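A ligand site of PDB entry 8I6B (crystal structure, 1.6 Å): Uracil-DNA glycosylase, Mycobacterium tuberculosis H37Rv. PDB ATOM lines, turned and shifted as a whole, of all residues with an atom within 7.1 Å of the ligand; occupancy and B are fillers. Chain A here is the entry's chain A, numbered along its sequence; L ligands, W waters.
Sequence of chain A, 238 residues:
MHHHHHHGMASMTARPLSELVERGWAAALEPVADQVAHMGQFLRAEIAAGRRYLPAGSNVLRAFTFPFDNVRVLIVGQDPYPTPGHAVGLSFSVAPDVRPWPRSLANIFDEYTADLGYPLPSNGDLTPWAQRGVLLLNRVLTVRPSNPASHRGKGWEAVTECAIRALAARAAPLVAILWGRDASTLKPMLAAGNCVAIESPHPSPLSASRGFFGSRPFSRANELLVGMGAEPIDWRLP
A ring nitrogen (NE2) of His 202 sits at hydrogen-bond distance from an oxygen (O2) of the ligand, 2.8 Å away.
OD1 of Asn 138 lies within hydrogen-bond range of N1 of the ligand (2.9 Å).
N1 of the ligand is in hydrogen-bond range of O of Asp 79 (2.8 Å).
The backbone NH (N) of Phe 92 lies within hydrogen-bond range of an oxygen (O1) of the ligand (2.9 Å).
The backbone NH (N) of Gln 78 is in hydrogen-bond range of an oxygen (O2) of the ligand.
The side-chain hydroxyl (OH) of Tyr 81 lies within hydrogen-bond range of the backbone carbonyl oxygen (O) of Phe 92.
O of Leu 136 lies within hydrogen-bond range of N of Ser 91 (2.9 Å).
O of Gln 78 is in hydrogen-bond range of N of Val 140 (3.0 Å).
The backbone carbonyl oxygen (O) of Gln 78 is in hydrogen-bond range of the backbone NH (N) of Arg 139, 3.3 Å away.
The backbone carbonyl oxygen (O) of Gly 77 is in hydrogen-bond range of the backbone NH (N) of Arg 139 (2.8 Å).
ND1 of His 202 is in hydrogen-bond range of N of Ser 204 (2.9 Å).
The backbone NH of Gln 78 lies within hydrogen-bond range of the side-chain amide oxygen of Asn 138 (3.5 Å).
N of Gly 77 is in hydrogen-bond range of O of Leu 137 (2.9 Å).
CA of Gly 77 touches O2 of the ligand, at 3.7 Å.
Pro 80 touches the ligand (CA to O1, 3.9 Å).
Tyr 81 touches the ligand.
Ser 91 touches the ligand (CA to O1, 3.4 Å).
Hydrophobic or aromatic side chains within 4 Å of the ligand: Tyr 81, Phe 92 and His 202.
Within 4 Å of the ligand: Gly 77, Gln 78, Asp 79, Pro 80, Tyr 81, Ser 91, Phe 92, Asn 138 and His 202.
The nearest printed residue that does not touch the ligand is Ser 104 (4.3 Å).
Water W1 lies within hydrogen-bond range of O3 of the ligand and OG of Ser 104.
Water W3 lies within hydrogen-bond range of O3 of the ligand (2.6 Å), OD1 of Asp 79 (2.9 Å) and NE2 of Gln 78 (3.2 Å).
Water W2 bridges an oxygen (O1) of the ligand and the backbone NH of Tyr 81.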
ATOM      1  N   VAL A  76      -0.213 -11.988   7.548  1.00  0.00           N
ATOM      2  CA  VAL A  76      -0.605 -11.935   8.984  1.00  0.00           C
ATOM      3  C   VAL A  76       0.438 -11.121   9.732  1.00  0.00           C
ATOM      4  O   VAL A  76       1.637 -11.526   9.797  1.00  0.00           O
ATOM      5  CB  VAL A  76      -0.831 -13.314   9.589  1.00  0.00           C
ATOM      6  CG1 VAL A  76      -1.503 -13.201  10.940  1.00  0.00           C
ATOM      7  CG2 VAL A  76      -1.699 -14.186   8.678  1.00  0.00           C
ATOM      8  N   GLY A  77      -0.049 -10.071  10.396  1.00  0.00           N
ATOM      9  CA  GLY A  77       0.769  -9.387  11.397  1.00  0.00           C
ATOM     10  C   GLY A  77       0.339  -9.723  12.814  1.00  0.00           C
ATOM     11  O   GLY A  77      -0.368 -10.716  13.066  1.00  0.00           O
ATOM     12  N   GLN A  78       0.746  -8.880  13.720  1.00  0.00           N
ATOM     13  CA  GLN A  78       0.516  -9.085  15.175  1.00  0.00           C
ATOM     14  C   GLN A  78      -0.869  -8.557  15.620  1.00  0.00           C
ATOM     15  O   GLN A  78      -1.699  -9.299  16.134  1.00  0.00           O
ATOM     16  CB  GLN A  78       1.659  -8.433  15.950  1.00  0.00           C
ATOM     17  CG  GLN A  78       1.437  -8.491  17.471  1.00  0.00           C
ATOM     18  CD  GLN A  78       2.605  -7.911  18.242  1.00  0.00           C
ATOM     19  OE1 GLN A  78       3.662  -8.515  18.343  1.00  0.00           O
ATOM     20  NE2 GLN A  78       2.439  -6.718  18.776  1.00  0.00           N
ATOM     21  N   ASP A  79      -1.058  -7.258  15.514  1.00  0.00           N
ATOM     22  CA  ASP A  79      -2.223  -6.527  16.018  1.00  0.00           C
ATOM     23  C   ASP A  79      -2.255  -5.174  15.324  1.00  0.00           C
ATOM     24  O   ASP A  79      -1.272  -4.774  14.666  1.00  0.00           O
ATOM     25  CB  ASP A  79      -2.219  -6.441  17.552  1.00  0.00           C
ATOM     26  CG  ASP A  79      -1.165  -5.587  18.236  1.00  0.00           C
ATOM     27  OD1 ASP A  79      -0.083  -5.395  17.647  1.00  0.00           O
ATOM     28  OD2 ASP A  79      -1.452  -5.139  19.368  1.00  0.00           O
ATOM     29  N   PRO A  80      -3.394  -4.461  15.422  1.00  0.00           N
ATOM     30  CA  PRO A  80      -3.501  -3.195  14.724  1.00  0.00           C
ATOM     31  C   PRO A  80      -2.545  -2.102  15.199  1.00  0.00           C
ATOM     32  O   PRO A  80      -1.965  -2.146  16.269  1.00  0.00           O
ATOM     33  CB  PRO A  80      -4.959  -2.740  14.953  1.00  0.00           C
ATOM     34  CG  PRO A  80      -5.664  -4.090  15.260  1.00  0.00           C
ATOM     35  CD  PRO A  80      -4.625  -4.795  16.132  1.00  0.00           C
ATOM     36  N   TYR A  81      -2.384  -1.119  14.321  1.00  0.00           N
ATOM     37  CA  TYR A  81      -1.571   0.072  14.663  1.00  0.00           C
ATOM     38  C   TYR A  81      -2.134   0.635  15.958  1.00  0.00           C
ATOM     39  O   TYR A  81      -3.326   0.807  16.065  1.00  0.00           O
ATOM     40  CB  TYR A  81      -1.630   1.128  13.568  1.00  0.00           C
ATOM     41  CG  TYR A  81      -0.869   0.769  12.310  1.00  0.00           C
ATOM     42  CD1 TYR A  81       0.504   0.584  12.320  1.00  0.00           C
ATOM     43  CD2 TYR A  81      -1.542   0.619  11.110  1.00  0.00           C
ATOM     44  CE1 TYR A  81       1.195   0.289  11.158  1.00  0.00           C
ATOM     45  CE2 TYR A  81      -0.863   0.360   9.929  1.00  0.00           C
ATOM     46  CZ  TYR A  81       0.521   0.162   9.966  1.00  0.00           C
ATOM     47  OH  TYR A  81       1.224  -0.126   8.821  1.00  0.00           O
ATOM     48  N   PRO A  82      -1.264   1.040  16.919  1.00  0.00           N
ATOM     49  CA  PRO A  82      -1.738   1.583  18.196  1.00  0.00           C
ATOM     50  C   PRO A  82      -1.992   3.083  18.188  1.00  0.00           C
ATOM     51  O   PRO A  82      -2.499   3.575  19.201  1.00  0.00           O
ATOM     52  CB  PRO A  82      -0.562   1.216  19.080  1.00  0.00           C
ATOM     53  CG  PRO A  82       0.671   1.432  18.201  1.00  0.00           C
ATOM     54  CD  PRO A  82       0.178   0.829  16.898  1.00  0.00           C
ATOM     55  N   ALA A  87      -5.077   2.569  12.232  1.00  0.00           N
ATOM     56  CA  ALA A  87      -5.649   1.238  11.926  1.00  0.00           C
ATOM     57  C   ALA A  87      -6.987   1.407  11.212  1.00  0.00           C
ATOM     58  O   ALA A  87      -7.835   2.243  11.679  1.00  0.00           O
ATOM     59  CB  ALA A  87      -5.776   0.447  13.187  1.00  0.00           C
ATOM     60  N   VAL A  88      -7.186   0.626  10.161  1.00  0.00           N
ATOM     61  CA  VAL A  88      -8.411   0.652   9.321  1.00  0.00           C
ATOM     62  C   VAL A  88      -9.039  -0.725   9.170  1.00  0.00           C
ATOM     63  O   VAL A  88     -10.003  -0.855   8.429  1.00  0.00           O
ATOM     64  CB  VAL A  88      -8.124   1.271   7.947  1.00  0.00           C
ATOM     65  CG1 VAL A  88      -7.727   2.734   8.106  1.00  0.00           C
ATOM     66  CG2 VAL A  88      -7.146   0.484   7.121  1.00  0.00           C
ATOM     67  N   GLY A  89      -8.544  -1.750   9.870  1.00  0.00           N
ATOM     68  CA  GLY A  89      -9.144  -3.093   9.857  1.00  0.00           C
ATOM     69  C   GLY A  89      -8.533  -3.989   8.810  1.00  0.00           C
ATOM     70  O   GLY A  89      -8.984  -5.127   8.708  1.00  0.00           O
ATOM     71  N   LEU A  90      -7.623  -3.473   7.987  1.00  0.00           N
ATOM     72  CA  LEU A  90      -6.798  -4.261   7.035  1.00  0.00           C
ATOM     73  C   LEU A  90      -5.368  -4.155   7.504  1.00  0.00           C
ATOM     74  O   LEU A  90      -4.857  -3.029   7.718  1.00  0.00           O
ATOM     75  CB  LEU A  90      -6.913  -3.689   5.624  1.00  0.00           C
ATOM     76  CG  LEU A  90      -8.315  -3.754   5.017  1.00  0.00           C
ATOM     77  CD1 LEU A  90      -8.323  -3.024   3.695  1.00  0.00           C
ATOM     78  CD2 LEU A  90      -8.819  -5.171   4.877  1.00  0.00           C
ATOM     79  N   SER A  91      -4.747  -5.293   7.832  1.00  0.00           N
ATOM     80  CA  SER A  91      -3.427  -5.234   8.486  1.00  0.00           C
ATOM     81  C   SER A  91      -2.462  -4.395   7.658  1.00  0.00           C
ATOM     82  O   SER A  91      -2.475  -4.443   6.445  1.00  0.00           O
ATOM     83  CB  SER A  91      -2.900  -6.618   8.792  1.00  0.00           C
ATOM     84  OG  SER A  91      -2.665  -7.371   7.639  1.00  0.00           O
ATOM     85  N   PHE A  92      -1.685  -3.564   8.346  1.00  0.00           N
ATOM     86  CA  PHE A  92      -0.639  -2.664   7.820  1.00  0.00           C
ATOM     87  C   PHE A  92      -1.180  -1.494   6.989  1.00  0.00           C
ATOM     88  O   PHE A  92      -0.427  -0.532   6.792  1.00  0.00           O
ATOM     89  CB  PHE A  92       0.447  -3.476   7.135  1.00  0.00           C
ATOM     90  CG  PHE A  92       1.093  -4.439   8.089  1.00  0.00           C
ATOM     91  CD1 PHE A  92       2.031  -4.009   9.011  1.00  0.00           C
ATOM     92  CD2 PHE A  92       0.761  -5.775   8.045  1.00  0.00           C
ATOM     93  CE1 PHE A  92       2.603  -4.925   9.876  1.00  0.00           C
ATOM     94  CE2 PHE A  92       1.346  -6.707   8.920  1.00  0.00           C
ATOM     95  CZ  PHE A  92       2.211  -6.265   9.874  1.00  0.00           C
ATOM     96  N   SER A  93      -2.424  -1.518   6.600  1.00  0.00           N
ATOM     97  CA  SER A  93      -2.966  -0.472   5.723  1.00  0.00           C
ATOM     98  C   SER A  93      -3.238   0.813   6.504  1.00  0.00           C
ATOM     99  O   SER A  93      -3.579   0.737   7.718  1.00  0.00           O
ATOM    100  CB  SER A  93      -4.209  -0.972   5.051  1.00  0.00           C
ATOM    101  OG  SER A  93      -4.556  -0.125   3.969  1.00  0.00           O
ATOM    102  N   PRO A 102       3.364   4.943   9.043  1.00  0.00           N
ATOM    103  CA  PRO A 102       3.907   4.216  10.181  1.00  0.00           C
ATOM    104  C   PRO A 102       5.246   3.579   9.772  1.00  0.00           C
ATOM    105  O   PRO A 102       5.397   3.179   8.627  1.00  0.00           O
ATOM    106  CB  PRO A 102       2.836   3.170  10.505  1.00  0.00           C
ATOM    107  CG  PRO A 102       1.556   3.764   9.952  1.00  0.00           C
ATOM    108  CD  PRO A 102       1.993   4.500   8.703  1.00  0.00           C
ATOM    109  N   SER A 104       6.636   0.678  10.398  1.00  0.00           N
ATOM    110  CA  SER A 104       6.498  -0.698   9.879  1.00  0.00           C
ATOM    111  C   SER A 104       6.112  -0.662   8.404  1.00  0.00           C
ATOM    112  O   SER A 104       6.578  -1.510   7.643  1.00  0.00           O
ATOM    113  CB  SER A 104       5.493  -1.522  10.648  1.00  0.00           C
ATOM    114  OG  SER A 104       6.017  -1.856  11.911  1.00  0.00           O
ATOM    115  N   LEU A 105       5.222   0.242   8.030  1.00  0.00           N
ATOM    116  CA  LEU A 105       4.739   0.316   6.635  1.00  0.00           C
ATOM    117  C   LEU A 105       5.837   0.858   5.753  1.00  0.00           C
ATOM    118  O   LEU A 105       5.990   0.383   4.649  1.00  0.00           O
ATOM    119  CB  LEU A 105       3.467   1.154   6.538  1.00  0.00           C
ATOM    120  CG  LEU A 105       2.810   1.121   5.163  1.00  0.00           C
ATOM    121  CD1 LEU A 105       2.374  -0.271   4.773  1.00  0.00           C
ATOM    122  CD2 LEU A 105       1.624   2.072   5.120  1.00  0.00           C
ATOM    123  N   LEU A 136      -5.568  -9.387   4.493  1.00  0.00           N
ATOM    124  CA  LEU A 136      -4.710  -8.543   5.338  1.00  0.00           C
ATOM    125  C   LEU A 136      -5.138  -8.716   6.782  1.00  0.00           C
ATOM    126  O   LEU A 136      -5.938  -7.918   7.312  1.00  0.00           O
ATOM    127  CB  LEU A 136      -4.759  -7.098   4.863  1.00  0.00           C
ATOM    128  CG  LEU A 136      -4.218  -6.909   3.443  1.00  0.00           C
ATOM    129  CD1 LEU A 136      -4.373  -5.461   2.989  1.00  0.00           C
ATOM    130  CD2 LEU A 136      -2.778  -7.303   3.362  1.00  0.00           C
ATOM    131  N   LEU A 137      -4.622  -9.749   7.396  1.00  0.00           N
ATOM    132  CA  LEU A 137      -5.055 -10.180   8.752  1.00  0.00           C
ATOM    133  C   LEU A 137      -4.023  -9.796   9.800  1.00  0.00           C
ATOM    134  O   LEU A 137      -2.808  -9.625   9.518  1.00  0.00           O
ATOM    135  CB  LEU A 137      -5.218 -11.702   8.722  1.00  0.00           C
ATOM    136  CG  LEU A 137      -6.048 -12.327   9.827  1.00  0.00           C
ATOM    137  CD1 LEU A 137      -7.453 -11.810   9.845  1.00  0.00           C
ATOM    138  CD2 LEU A 137      -6.004 -13.861   9.752  1.00  0.00           C
ATOM    139  N   ASN A 138      -4.471  -9.672  11.038  1.00  0.00           N
ATOM    140  CA  ASN A 138      -3.628  -9.599  12.241  1.00  0.00           C
ATOM    141  C   ASN A 138      -3.993 -10.795  13.117  1.00  0.00           C
ATOM    142  O   ASN A 138      -5.179 -11.191  13.078  1.00  0.00           O
ATOM    143  CB  ASN A 138      -3.796  -8.290  12.986  1.00  0.00           C
ATOM    144  CG  ASN A 138      -3.016  -7.170  12.339  1.00  0.00           C
ATOM    145  OD1 ASN A 138      -1.862  -7.360  11.985  1.00  0.00           O
ATOM    146  ND2 ASN A 138      -3.644  -6.005  12.193  1.00  0.00           N
ATOM    147  N   ARG A 139      -3.021 -11.338  13.852  1.00  0.00           N
ATOM    148  CA  ARG A 139      -3.337 -12.441  14.788  1.00  0.00           C
ATOM    149  C   ARG A 139      -4.406 -11.989  15.788  1.00  0.00           C
ATOM    150  O   ARG A 139      -5.301 -12.816  16.169  1.00  0.00           O
ATOM    151  CB  ARG A 139      -2.059 -12.917  15.509  1.00  0.00           C
ATOM    152  CG  ARG A 139      -2.245 -14.226  16.253  1.00  0.00           C
ATOM    153  CD  ARG A 139      -2.352 -15.417  15.321  1.00  0.00           C
ATOM    154  NE  ARG A 139      -2.270 -16.657  16.065  1.00  0.00           N
ATOM    155  CZ  ARG A 139      -3.299 -17.325  16.609  1.00  0.00           C
ATOM    156  NH1 ARG A 139      -4.575 -17.028  16.338  1.00  0.00           N
ATOM    157  NH2 ARG A 139      -3.013 -18.379  17.372  1.00  0.00           N
ATOM    158  N   VAL A 140      -4.349 -10.739  16.226  1.00  0.00           N
ATOM    159  CA  VAL A 140      -5.308 -10.127  17.176  1.00  0.00           C
ATOM    160  C   VAL A 140      -5.895  -8.881  16.517  1.00  0.00           C
ATOM    161  O   VAL A 140      -5.142  -8.161  15.836  1.00  0.00           O
ATOM    162  CB  VAL A 140      -4.558  -9.816  18.493  1.00  0.00           C
ATOM    163  CG1 VAL A 140      -5.364  -8.903  19.374  1.00  0.00           C
ATOM    164  CG2 VAL A 140      -4.179 -11.113  19.207  1.00  0.00           C
ATOM    165  N   TRP A 179       4.363 -12.591   9.460  1.00  0.00           N
ATOM    166  CA  TRP A 179       5.290 -11.568   9.960  1.00  0.00           C
ATOM    167  C   TRP A 179       5.266 -11.507  11.479  1.00  0.00           C
ATOM    168  O   TRP A 179       4.283 -11.011  12.087  1.00  0.00           O
ATOM    169  CB  TRP A 179       4.983 -10.207   9.342  1.00  0.00           C
ATOM    170  CG  TRP A 179       5.381 -10.101   7.900  1.00  0.00           C
ATOM    171  CD1 TRP A 179       6.265 -10.869   7.232  1.00  0.00           C
ATOM    172  CD2 TRP A 179       4.802  -9.202   6.949  1.00  0.00           C
ATOM    173  NE1 TRP A 179       6.341 -10.470   5.910  1.00  0.00           N
ATOM    174  CE2 TRP A 179       5.485  -9.422   5.734  1.00  0.00           C
ATOM    175  CE3 TRP A 179       3.859  -8.162   7.019  1.00  0.00           C
ATOM    176  CZ2 TRP A 179       5.154  -8.705   4.580  1.00  0.00           C
ATOM    177  CZ3 TRP A 179       3.551  -7.469   5.877  1.00  0.00           C
ATOM    178  CH2 TRP A 179       4.211  -7.732   4.684  1.00  0.00           C
ATOM    179  N   HIS A 202       9.072  -9.666  11.850  1.00  0.00           N
ATOM    180  CA  HIS A 202       8.102  -8.588  11.624  1.00  0.00           C
ATOM    181  C   HIS A 202       8.818  -7.357  11.101  1.00  0.00           C
ATOM    182  O   HIS A 202       9.953  -7.081  11.466  1.00  0.00           O
ATOM    183  CB  HIS A 202       7.405  -8.356  12.954  1.00  0.00           C
ATOM    184  CG  HIS A 202       6.243  -7.434  12.947  1.00  0.00           C
ATOM    185  ND1 HIS A 202       6.371  -6.084  12.895  1.00  0.00           N
ATOM    186  CD2 HIS A 202       4.928  -7.689  13.051  1.00  0.00           C
ATOM    187  CE1 HIS A 202       5.198  -5.505  12.917  1.00  0.00           C
ATOM    188  NE2 HIS A 202       4.256  -6.472  13.011  1.00  0.00           N
ATOM    189  N   PRO A 203       8.133  -6.553  10.262  1.00  0.00           N
ATOM    190  CA  PRO A 203       8.738  -5.344   9.680  1.00  0.00           C
ATOM    191  C   PRO A 203       8.909  -4.143  10.617  1.00  0.00           C
ATOM    192  O   PRO A 203       9.439  -3.106  10.261  1.00  0.00           O
ATOM    193  CB  PRO A 203       7.771  -5.015   8.516  1.00  0.00           C
ATOM    194  CG  PRO A 203       6.457  -5.544   9.008  1.00  0.00           C
ATOM    195  CD  PRO A 203       6.815  -6.842   9.685  1.00  0.00           C
ATOM    196  N   SER A 204       8.461  -4.280  11.861  1.00  0.00           N
ATOM    197  CA  SER A 204       8.716  -3.270  12.916  1.00  0.00           C
ATOM    198  C   SER A 204      10.191  -2.952  12.980  1.00  0.00           C
ATOM    199  O   SER A 204      11.008  -3.858  12.849  1.00  0.00           O
ATOM    200  CB  SER A 204       8.290  -3.803  14.229  1.00  0.00           C
ATOM    201  OG  SER A 204       8.816  -2.994  15.280  1.00  0.00           O
HETATM  202  O1  LIG L   1      -1.886  -3.849  11.210  1.00  0.00           O
HETATM  203  C1  LIG L   1      -0.852  -3.861  11.769  1.00  0.00           C
HETATM  204  N1  LIG L   1      -0.199  -5.029  12.087  1.00  0.00           N
HETATM  205  C2  LIG L   1       0.967  -5.134  12.800  1.00  0.00           C
HETATM  206  O2  LIG L   1       1.458  -6.197  13.112  1.00  0.00           O
HETATM  207  N2  LIG L   1      -0.188  -2.685  12.041  1.00  0.00           N
HETATM  208  C3  LIG L   1       1.077  -2.667  12.785  1.00  0.00           C
HETATM  209  C4  LIG L   1       1.640  -3.873  13.066  1.00  0.00           C
HETATM  210  O3  LIG L   1       2.791  -3.916  13.786  1.00  0.00           O
HETATM  211  O   HOH W   1       4.303  -1.966  13.852  1.00  0.00           O
HETATM  212  O   HOH W   2      -3.729  -1.866  11.708  1.00  0.00           O
HETATM  213  O   HOH W   3       2.304  -4.786  16.207  1.00  0.00           O
